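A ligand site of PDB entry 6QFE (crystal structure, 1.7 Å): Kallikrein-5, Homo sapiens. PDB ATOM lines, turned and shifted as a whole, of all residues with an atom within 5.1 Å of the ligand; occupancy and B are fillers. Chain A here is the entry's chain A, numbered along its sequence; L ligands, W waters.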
ATOM      1  N   HIS A  42     -12.563  -7.249  -3.406  1.00  0.00           N
ATOM      2  CA  HIS A  42     -13.215  -6.335  -2.458  1.00  0.00           C
ATOM      3  C   HIS A  42     -12.796  -4.870  -2.691  1.00  0.00           C
ATOM      4  O   HIS A  42     -13.402  -3.959  -2.093  1.00  0.00           O
ATOM      5  CB  HIS A  42     -13.025  -6.754  -0.980  1.00  0.00           C
ATOM      6  CG  HIS A  42     -11.673  -6.479  -0.402  1.00  0.00           C
ATOM      7  ND1 HIS A  42     -10.744  -7.480  -0.260  1.00  0.00           N
ATOM      8  CD2 HIS A  42     -11.157  -5.335   0.119  1.00  0.00           C
ATOM      9  CE1 HIS A  42      -9.673  -6.908   0.281  1.00  0.00           C
ATOM     10  NE2 HIS A  42      -9.882  -5.625   0.520  1.00  0.00           N
ATOM     11  N   TYR A  79     -16.792 -14.731  -6.748  1.00  0.00           N
ATOM     12  CA  TYR A  79     -16.787 -13.735  -5.678  1.00  0.00           C
ATOM     13  C   TYR A  79     -18.256 -13.252  -5.497  1.00  0.00           C
ATOM     14  O   TYR A  79     -18.976 -13.057  -6.462  1.00  0.00           O
ATOM     15  CB  TYR A  79     -15.915 -12.514  -6.113  1.00  0.00           C
ATOM     16  CG  TYR A  79     -15.827 -11.441  -5.058  1.00  0.00           C
ATOM     17  CD1 TYR A  79     -15.116 -11.650  -3.874  1.00  0.00           C
ATOM     18  CD2 TYR A  79     -16.510 -10.219  -5.210  1.00  0.00           C
ATOM     19  CE1 TYR A  79     -15.037 -10.656  -2.887  1.00  0.00           C
ATOM     20  CE2 TYR A  79     -16.472  -9.239  -4.207  1.00  0.00           C
ATOM     21  CZ  TYR A  79     -15.741  -9.468  -3.047  1.00  0.00           C
ATOM     22  OH  TYR A  79     -15.653  -8.528  -2.060  1.00  0.00           O
ATOM     23  N   HIS A  81     -19.700 -10.306  -2.999  1.00  0.00           N
ATOM     24  CA  HIS A  81     -19.531  -9.268  -1.971  1.00  0.00           C
ATOM     25  C   HIS A  81     -20.674  -9.343  -0.928  1.00  0.00           C
ATOM     26  O   HIS A  81     -21.831  -9.503  -1.317  1.00  0.00           O
ATOM     27  CB  HIS A  81     -19.516  -7.876  -2.619  1.00  0.00           C
ATOM     28  CG  HIS A  81     -18.939  -6.804  -1.738  1.00  0.00           C
ATOM     29  ND1 HIS A  81     -17.575  -6.712  -1.508  1.00  0.00           N
ATOM     30  CD2 HIS A  81     -19.567  -5.817  -1.052  1.00  0.00           C
ATOM     31  CE1 HIS A  81     -17.406  -5.667  -0.717  1.00  0.00           C
ATOM     32  NE2 HIS A  81     -18.587  -5.096  -0.409  1.00  0.00           N
ATOM     33  N   PRO A  82     -20.393  -9.267   0.400  1.00  0.00           N
ATOM     34  CA  PRO A  82     -19.097  -9.028   1.075  1.00  0.00           C
ATOM     35  C   PRO A  82     -18.328 -10.274   1.516  1.00  0.00           C
ATOM     36  O   PRO A  82     -17.412 -10.147   2.336  1.00  0.00           O
ATOM     37  CB  PRO A  82     -19.502  -8.178   2.280  1.00  0.00           C
ATOM     38  CG  PRO A  82     -20.848  -8.782   2.680  1.00  0.00           C
ATOM     39  CD  PRO A  82     -21.492  -9.301   1.386  1.00  0.00           C
ATOM     40  N   HIS A  84     -15.612 -13.364   1.705  1.00  0.00           N
ATOM     41  CA  HIS A  84     -14.167 -13.404   1.421  1.00  0.00           C
ATOM     42  C   HIS A  84     -13.719 -14.369   0.314  1.00  0.00           C
ATOM     43  O   HIS A  84     -12.619 -14.201  -0.199  1.00  0.00           O
ATOM     44  CB  HIS A  84     -13.353 -13.704   2.686  1.00  0.00           C
ATOM     45  CG  HIS A  84     -13.487 -12.679   3.761  1.00  0.00           C
ATOM     46  ND1 HIS A  84     -13.183 -11.356   3.534  1.00  0.00           N
ATOM     47  CD2 HIS A  84     -13.822 -12.834   5.056  1.00  0.00           C
ATOM     48  CE1 HIS A  84     -13.362 -10.748   4.688  1.00  0.00           C
ATOM     49  NE2 HIS A  84     -13.758 -11.597   5.632  1.00  0.00           N
ATOM     50  N   SER A 129      -1.682  -0.678  14.146  1.00  0.00           N
ATOM     51  CA  SER A 129      -3.063  -1.112  14.311  1.00  0.00           C
ATOM     52  C   SER A 129      -3.288  -1.301  15.815  1.00  0.00           C
ATOM     53  O   SER A 129      -2.442  -1.916  16.440  1.00  0.00           O
ATOM     54  CB  SER A 129      -3.351  -2.407  13.555  1.00  0.00           C
ATOM     55  OG  SER A 129      -4.726  -2.710  13.671  1.00  0.00           O
ATOM     56  N   ASP A 173       2.140  -8.492  10.406  1.00  0.00           N
ATOM     57  CA  ASP A 173       0.971  -8.778   9.562  1.00  0.00           C
ATOM     58  C   ASP A 173       0.827  -7.712   8.506  1.00  0.00           C
ATOM     59  O   ASP A 173       1.482  -6.652   8.561  1.00  0.00           O
ATOM     60  CB  ASP A 173      -0.303  -8.737  10.471  1.00  0.00           C
ATOM     61  CG  ASP A 173      -1.590  -9.425   9.996  1.00  0.00           C
ATOM     62  OD1 ASP A 173      -1.566 -10.054   8.940  1.00  0.00           O
ATOM     63  OD2 ASP A 173      -2.646  -9.216  10.637  1.00  0.00           O
ATOM     64  N   SER A 174      -0.074  -7.957   7.517  1.00  0.00           N
ATOM     65  CA  SER A 174      -0.464  -6.941   6.556  1.00  0.00           C
ATOM     66  C   SER A 174      -1.673  -6.301   7.276  1.00  0.00           C
ATOM     67  O   SER A 174      -2.066  -6.795   8.343  1.00  0.00           O
ATOM     68  CB  SER A 174      -0.857  -7.548   5.198  1.00  0.00           C
ATOM     69  OG  SER A 174      -1.851  -8.544   5.363  1.00  0.00           O
ATOM     70  N   CYS A 175      -2.182  -5.184   6.775  1.00  0.00           N
ATOM     71  CA  CYS A 175      -3.259  -4.491   7.480  1.00  0.00           C
ATOM     72  C   CYS A 175      -4.093  -3.645   6.502  1.00  0.00           C
ATOM     73  O   CYS A 175      -3.858  -3.700   5.292  1.00  0.00           O
ATOM     74  CB  CYS A 175      -2.638  -3.637   8.583  1.00  0.00           C
ATOM     75  SG  CYS A 175      -3.782  -3.218   9.922  1.00  0.00           S
ATOM     76  N   GLN A 176      -5.027  -2.830   7.006  1.00  0.00           N
ATOM     77  CA  GLN A 176      -5.836  -1.965   6.140  1.00  0.00           C
ATOM     78  C   GLN A 176      -4.981  -1.030   5.277  1.00  0.00           C
ATOM     79  O   GLN A 176      -3.957  -0.510   5.730  1.00  0.00           O
ATOM     80  CB  GLN A 176      -6.984  -1.221   6.887  1.00  0.00           C
ATOM     81  CG  GLN A 176      -6.665  -0.203   7.907  1.00  0.00           C
ATOM     82  CD  GLN A 176      -7.858   0.144   8.758  1.00  0.00           C
ATOM     83  OE1 GLN A 176      -7.689   0.297   9.936  1.00  0.00           O
ATOM     84  NE2 GLN A 176      -9.095   0.127   8.227  1.00  0.00           N
ATOM     85  N   GLY A 177      -5.379  -0.921   4.004  1.00  0.00           N
ATOM     86  CA  GLY A 177      -4.633  -0.156   3.019  1.00  0.00           C
ATOM     87  C   GLY A 177      -3.687  -1.054   2.236  1.00  0.00           C
ATOM     88  O   GLY A 177      -3.217  -0.644   1.182  1.00  0.00           O
ATOM     89  N   SER A 179      -4.665  -4.120   1.146  1.00  0.00           N
ATOM     90  CA  SER A 179      -5.567  -4.923   0.291  1.00  0.00           C
ATOM     91  C   SER A 179      -5.130  -5.008  -1.178  1.00  0.00           C
ATOM     92  O   SER A 179      -4.786  -4.006  -1.775  1.00  0.00           O
ATOM     93  CB  SER A 179      -6.965  -4.347   0.301  1.00  0.00           C
ATOM     94  OG  SER A 179      -7.591  -4.616   1.543  1.00  0.00           O
ATOM     95  N   VAL A 193      -3.188  -9.691  -0.711  1.00  0.00           N
ATOM     96  CA  VAL A 193      -3.632  -9.306   0.645  1.00  0.00           C
ATOM     97  C   VAL A 193      -5.172  -9.284   0.612  1.00  0.00           C
ATOM     98  O   VAL A 193      -5.757  -8.598  -0.222  1.00  0.00           O
ATOM     99  CB  VAL A 193      -3.094  -7.914   1.032  1.00  0.00           C
ATOM    100  CG1 VAL A 193      -3.628  -7.501   2.396  1.00  0.00           C
ATOM    101  CG2 VAL A 193      -1.561  -7.903   1.010  1.00  0.00           C
ATOM    102  N   SER A 194      -5.813 -10.125   1.436  1.00  0.00           N
ATOM    103  CA  SER A 194      -7.276 -10.200   1.410  1.00  0.00           C
ATOM    104  C   SER A 194      -7.866  -9.705   2.730  1.00  0.00           C
ATOM    105  O   SER A 194      -8.520  -8.661   2.732  1.00  0.00           O
ATOM    106  CB  SER A 194      -7.728 -11.629   1.105  1.00  0.00           C
ATOM    107  OG  SER A 194      -9.123 -11.719   0.905  1.00  0.00           O
ATOM    108  N   TRP A 195      -7.686 -10.443   3.836  1.00  0.00           N
ATOM    109  CA  TRP A 195      -8.306 -10.028   5.110  1.00  0.00           C
ATOM    110  C   TRP A 195      -7.555 -10.598   6.302  1.00  0.00           C
ATOM    111  O   TRP A 195      -6.420 -11.086   6.185  1.00  0.00           O
ATOM    112  CB  TRP A 195      -9.820 -10.458   5.129  1.00  0.00           C
ATOM    113  CG  TRP A 195     -10.053 -11.949   5.026  1.00  0.00           C
ATOM    114  CD1 TRP A 195     -10.019 -12.705   3.889  1.00  0.00           C
ATOM    115  CD2 TRP A 195     -10.515 -12.821   6.072  1.00  0.00           C
ATOM    116  NE1 TRP A 195     -10.356 -14.015   4.175  1.00  0.00           N
ATOM    117  CE2 TRP A 195     -10.671 -14.106   5.500  1.00  0.00           C
ATOM    118  CE3 TRP A 195     -10.785 -12.643   7.438  1.00  0.00           C
ATOM    119  CZ2 TRP A 195     -11.086 -15.224   6.266  1.00  0.00           C
ATOM    120  CZ3 TRP A 195     -11.169 -13.755   8.192  1.00  0.00           C
ATOM    121  CH2 TRP A 195     -11.313 -15.016   7.600  1.00  0.00           C
ATOM    122  N   GLY A 196      -8.189 -10.557   7.460  1.00  0.00           N
ATOM    123  CA  GLY A 196      -7.547 -11.051   8.673  1.00  0.00           C
ATOM    124  C   GLY A 196      -8.331 -10.558   9.848  1.00  0.00           C
ATOM    125  O   GLY A 196      -9.542 -10.355   9.737  1.00  0.00           O
ATOM    126  N   ASP A 197      -7.645 -10.285  10.947  1.00  0.00           N
ATOM    127  CA  ASP A 197      -8.339  -9.817  12.124  1.00  0.00           C
ATOM    128  C   ASP A 197      -7.959  -8.388  12.479  1.00  0.00           C
ATOM    129  O   ASP A 197      -6.988  -7.844  11.928  1.00  0.00           O
ATOM    130  CB  ASP A 197      -8.068 -10.781  13.295  1.00  0.00           C
ATOM    131  CG  ASP A 197      -9.287 -11.021  14.173  1.00  0.00           C
ATOM    132  OD1 ASP A 197     -10.139 -10.093  14.275  1.00  0.00           O
ATOM    133  OD2 ASP A 197      -9.382 -12.100  14.765  1.00  0.00           O
ATOM    134  N   TYR A 198      -8.775  -7.759  13.357  1.00  0.00           N
ATOM    135  CA  TYR A 198      -8.605  -6.419  13.877  1.00  0.00           C
ATOM    136  C   TYR A 198      -8.468  -6.461  15.415  1.00  0.00           C
ATOM    137  O   TYR A 198      -9.305  -7.077  16.073  1.00  0.00           O
ATOM    138  CB  TYR A 198      -9.828  -5.524  13.529  1.00  0.00           C
ATOM    139  CG  TYR A 198      -9.794  -4.153  14.203  1.00  0.00           C
ATOM    140  CD1 TYR A 198      -8.946  -3.148  13.731  1.00  0.00           C
ATOM    141  CD2 TYR A 198     -10.562  -3.887  15.346  1.00  0.00           C
ATOM    142  CE1 TYR A 198      -8.903  -1.903  14.356  1.00  0.00           C
ATOM    143  CE2 TYR A 198     -10.530  -2.645  15.962  1.00  0.00           C
ATOM    144  CZ  TYR A 198      -9.710  -1.649  15.460  1.00  0.00           C
ATOM    145  OH  TYR A 198      -9.647  -0.430  16.074  1.00  0.00           O
ATOM    146  N   CYS A 200      -4.765  -5.577  13.598  1.00  0.00           N
ATOM    147  CA  CYS A 200      -3.870  -6.457  12.829  1.00  0.00           C
ATOM    148  C   CYS A 200      -2.753  -6.950  13.728  1.00  0.00           C
ATOM    149  O   CYS A 200      -2.506  -6.338  14.769  1.00  0.00           O
ATOM    150  CB  CYS A 200      -3.304  -5.710  11.630  1.00  0.00           C
ATOM    151  SG  CYS A 200      -4.578  -4.968  10.579  1.00  0.00           S
ATOM    152  N   ALA A 201      -2.029  -8.007  13.295  1.00  0.00           N
ATOM    153  CA  ALA A 201      -0.832  -8.535  13.965  1.00  0.00           C
ATOM    154  C   ALA A 201      -1.062  -9.129  15.354  1.00  0.00           C
ATOM    155  O   ALA A 201      -0.120  -9.219  16.138  1.00  0.00           O
ATOM    156  CB  ALA A 201       0.264  -7.474  14.015  1.00  0.00           C
ATOM    157  N   GLY A 207      -2.678 -13.366   8.866  1.00  0.00           N
ATOM    158  CA  GLY A 207      -3.330 -12.714   7.732  1.00  0.00           C
ATOM    159  C   GLY A 207      -3.884 -13.782   6.808  1.00  0.00           C
ATOM    160  O   GLY A 207      -3.359 -14.919   6.740  1.00  0.00           O
ATOM    161  N   VAL A 208      -4.945 -13.451   6.110  1.00  0.00           N
ATOM    162  CA  VAL A 208      -5.612 -14.319   5.138  1.00  0.00           C
ATOM    163  C   VAL A 208      -5.403 -13.743   3.756  1.00  0.00           C
ATOM    164  O   VAL A 208      -5.672 -12.547   3.523  1.00  0.00           O
ATOM    165  CB  VAL A 208      -7.106 -14.629   5.423  1.00  0.00           C
ATOM    166  CG1 VAL A 208      -7.565 -15.796   4.560  1.00  0.00           C
ATOM    167  CG2 VAL A 208      -7.304 -14.965   6.909  1.00  0.00           C
ATOM    168  N   TYR A 209      -4.971 -14.603   2.843  1.00  0.00           N
ATOM    169  CA  TYR A 209      -4.548 -14.234   1.503  1.00  0.00           C
ATOM    170  C   TYR A 209      -5.269 -15.034   0.419  1.00  0.00           C
ATOM    171  O   TYR A 209      -5.589 -16.198   0.639  1.00  0.00           O
ATOM    172  CB  TYR A 209      -3.028 -14.454   1.429  1.00  0.00           C
ATOM    173  CG  TYR A 209      -2.290 -13.561   2.394  1.00  0.00           C
ATOM    174  CD1 TYR A 209      -2.020 -12.231   2.067  1.00  0.00           C
ATOM    175  CD2 TYR A 209      -1.950 -13.997   3.670  1.00  0.00           C
ATOM    176  CE1 TYR A 209      -1.441 -11.363   3.003  1.00  0.00           C
ATOM    177  CE2 TYR A 209      -1.352 -13.152   4.605  1.00  0.00           C
ATOM    178  CZ  TYR A 209      -1.081 -11.845   4.244  1.00  0.00           C
ATOM    179  OH  TYR A 209      -0.451 -11.018   5.133  1.00  0.00           O
HETATM  180  C1  LIG L   1     -10.314  -5.406   4.097  1.00  0.00           C
HETATM  181  C2  LIG L   1     -11.454  -6.983   3.202  1.00  0.00           C
HETATM  182  C3  LIG L   1     -13.768  -5.841   3.191  1.00  0.00           C
HETATM  183  C4  LIG L   1     -15.794  -4.532   3.117  1.00  0.00           C
HETATM  184  C5  LIG L   1     -14.459  -6.909   2.624  1.00  0.00           C
HETATM  185  C6  LIG L   1      -7.796  -6.318   6.498  1.00  0.00           C
HETATM  186  C7  LIG L   1      -7.077  -7.062   7.423  1.00  0.00           C
HETATM  187  C8  LIG L   1      -8.887  -7.066   9.066  1.00  0.00           C
HETATM  188  C9  LIG L   1     -10.270  -4.965   9.158  1.00  0.00           C
HETATM  189  C10 LIG L   1      -9.341  -2.986  10.076  1.00  0.00           C
HETATM  190  N1  LIG L   1      -5.075  -8.277   9.351  1.00  0.00           N
HETATM  191  C11 LIG L   1      -4.944  -8.346   8.004  1.00  0.00           C
HETATM  192  N2  LIG L   1      -3.989  -9.079   7.523  1.00  0.00           N
HETATM  193  C12 LIG L   1      -5.803  -7.566   7.103  1.00  0.00           C
HETATM  194  C13 LIG L   1      -5.276  -7.279   5.841  1.00  0.00           C
HETATM  195  C14 LIG L   1      -5.985  -6.523   4.922  1.00  0.00           C
HETATM  196  C15 LIG L   1      -7.229  -6.019   5.243  1.00  0.00           C
HETATM  197  N3  LIG L   1      -7.897  -5.232   4.326  1.00  0.00           N
HETATM  198  C16 LIG L   1      -9.165  -4.587   4.592  1.00  0.00           C
HETATM  199  N4  LIG L   1     -11.580  -4.944   4.016  1.00  0.00           N
HETATM  200  C17 LIG L   1     -12.322  -5.956   3.480  1.00  0.00           C
HETATM  201  N5  LIG L   1     -10.192  -6.633   3.599  1.00  0.00           N
HETATM  202  C18 LIG L   1     -14.450  -4.653   3.437  1.00  0.00           C
HETATM  203  C19 LIG L   1     -16.487  -5.608   2.586  1.00  0.00           C
HETATM  204  C20 LIG L   1     -15.803  -6.785   2.314  1.00  0.00           C
HETATM  205  O1  LIG L   1      -7.534  -7.363   8.683  1.00  0.00           O
HETATM  206  C21 LIG L   1      -9.066  -5.619   9.405  1.00  0.00           C
HETATM  207  C22 LIG L   1     -10.413  -3.632   9.509  1.00  0.00           C
HETATM  208  N6  LIG L   1      -8.154  -3.568  10.285  1.00  0.00           N
HETATM  209  C23 LIG L   1      -8.042  -4.873   9.976  1.00  0.00           C
HETATM  210  O   HOH W   1      -7.385  -2.245   2.714  1.00  0.00           O
HETATM  211  O   HOH W   2      -4.795 -10.806  11.397  1.00  0.00           O
HETATM  212  O   HOH W   3     -11.593  -8.238  10.397  1.00  0.00           O
HETATM  213  O   HOH W   4      -6.282  -1.762  11.709  1.00  0.00           O
HETATM  214  O   HOH W   5     -11.482  -7.644   6.643  1.00  0.00           O
HETATM  215  O   HOH W   6     -14.901  -9.222   0.321  1.00  0.00           O
HETATM  216  O   HOH W   7      -4.206 -10.326   4.638  1.00  0.00           O
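Residues that only touch the ligand: His 81 (3.4 Å), Pro 82 (3.7 Å), Cys 175 (3.6 Å), Gln 176 (3.6 Å), Val 193 (3.6 Å), Tyr 198 (3.6 Å) and Gly 207 (3.7 Å). Hydrophobic or aromatic side chains within 4 Å of the ligand: His 42, His 81, Pro 82, Val 193 and Tyr 198. The nearest printed residue that does not touch the ligand is His 84 (4.5 Å).
O of Asp 197 lies within hydrogen-bond range of N1 of the ligand (3.2 Å). N5 of the ligand lies within hydrogen-bond range of NE2 of His 42. The side-chain hydroxyl (OG) of Ser 179 sits at hydrogen-bond distance from a nitrogen (N3) of the ligand, 2.9 Å away. SG of Cys 200 lies close to N1 of the ligand (3.6 Å). An oxygen (O1) of the ligand is in hydrogen-bond range of the backbone NH of Gly 196. The backbone carbonyl oxygen of Trp 195 sits at hydrogen-bond distance from a nitrogen (N2) of the ligand (3.4 Å). A nitrogen (N2) of the ligand lies within hydrogen-bond range of the backbone carbonyl oxygen (O) of Ser 174, at 3.1 Å. O of Ser 194 sits close to N5 of the ligand, 2.8 Å away. N2 of the ligand sits at hydrogen-bond distance from OG of Ser 174. The side-chain carboxylate (OD2) of Asp 173 lies within salt-bridge range of a nitrogen (N1) of the ligand (2.9 Å).
A ring nitrogen (NE2) of His 42 sits at hydrogen-bond distance from the side-chain hydroxyl (OG) of Ser 179 (2.7 Å). The backbone NH of Ser 194 lies within hydrogen-bond range of the backbone carbonyl oxygen of Val 208, at 3.2 Å. The side-chain hydroxyl (OG) of Ser 129 sits at hydrogen-bond distance from the backbone NH (N) of Cys 200 (2.9 Å). O of Trp 195 lies within hydrogen-bond range of N of Val 208 (2.8 Å). OD2 of Asp 173 sits at hydrogen-bond distance from N of Ala 201. The side-chain sulfur of Cys 200 is disulfide-bonded to the side-chain sulfur of Cys 175 (2.0 Å). A ring nitrogen (ND1) of His 81 is in hydrogen-bond range of the side-chain hydroxyl (OH) of Tyr 79 (2.7 Å). The side-chain carboxylate (OD1) of Asp 173 lies close to the backbone NH (N) of Gly 207, at 3.5 Å.
Water W7 lies within hydrogen-bond range of the backbone carbonyl oxygen (O) of Trp 195 (2.8 Å), the backbone carbonyl oxygen (O) of Val 208 (2.9 Å), the side-chain hydroxyl (OG) of Ser 174 (3.0 Å) and a nitrogen (N2) of the ligand (3.2 Å). Water W2 lies within hydrogen-bond range of OD2 of Asp 173 (2.8 Å), N of Asp 197 (2.9 Å) and N1 of the ligand (3.3 Å). Water W6 lies within hydrogen-bond range of the side-chain hydroxyl (OH) of Tyr 79 and the backbone carbonyl oxygen (O) of Pro 82. Water W1 lies within hydrogen-bond range of the side-chain hydroxyl of Ser 179 (2.7 Å), the backbone NH of Gly 177 (2.7 Å) and a nitrogen (N3) of the ligand (3.4 Å).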
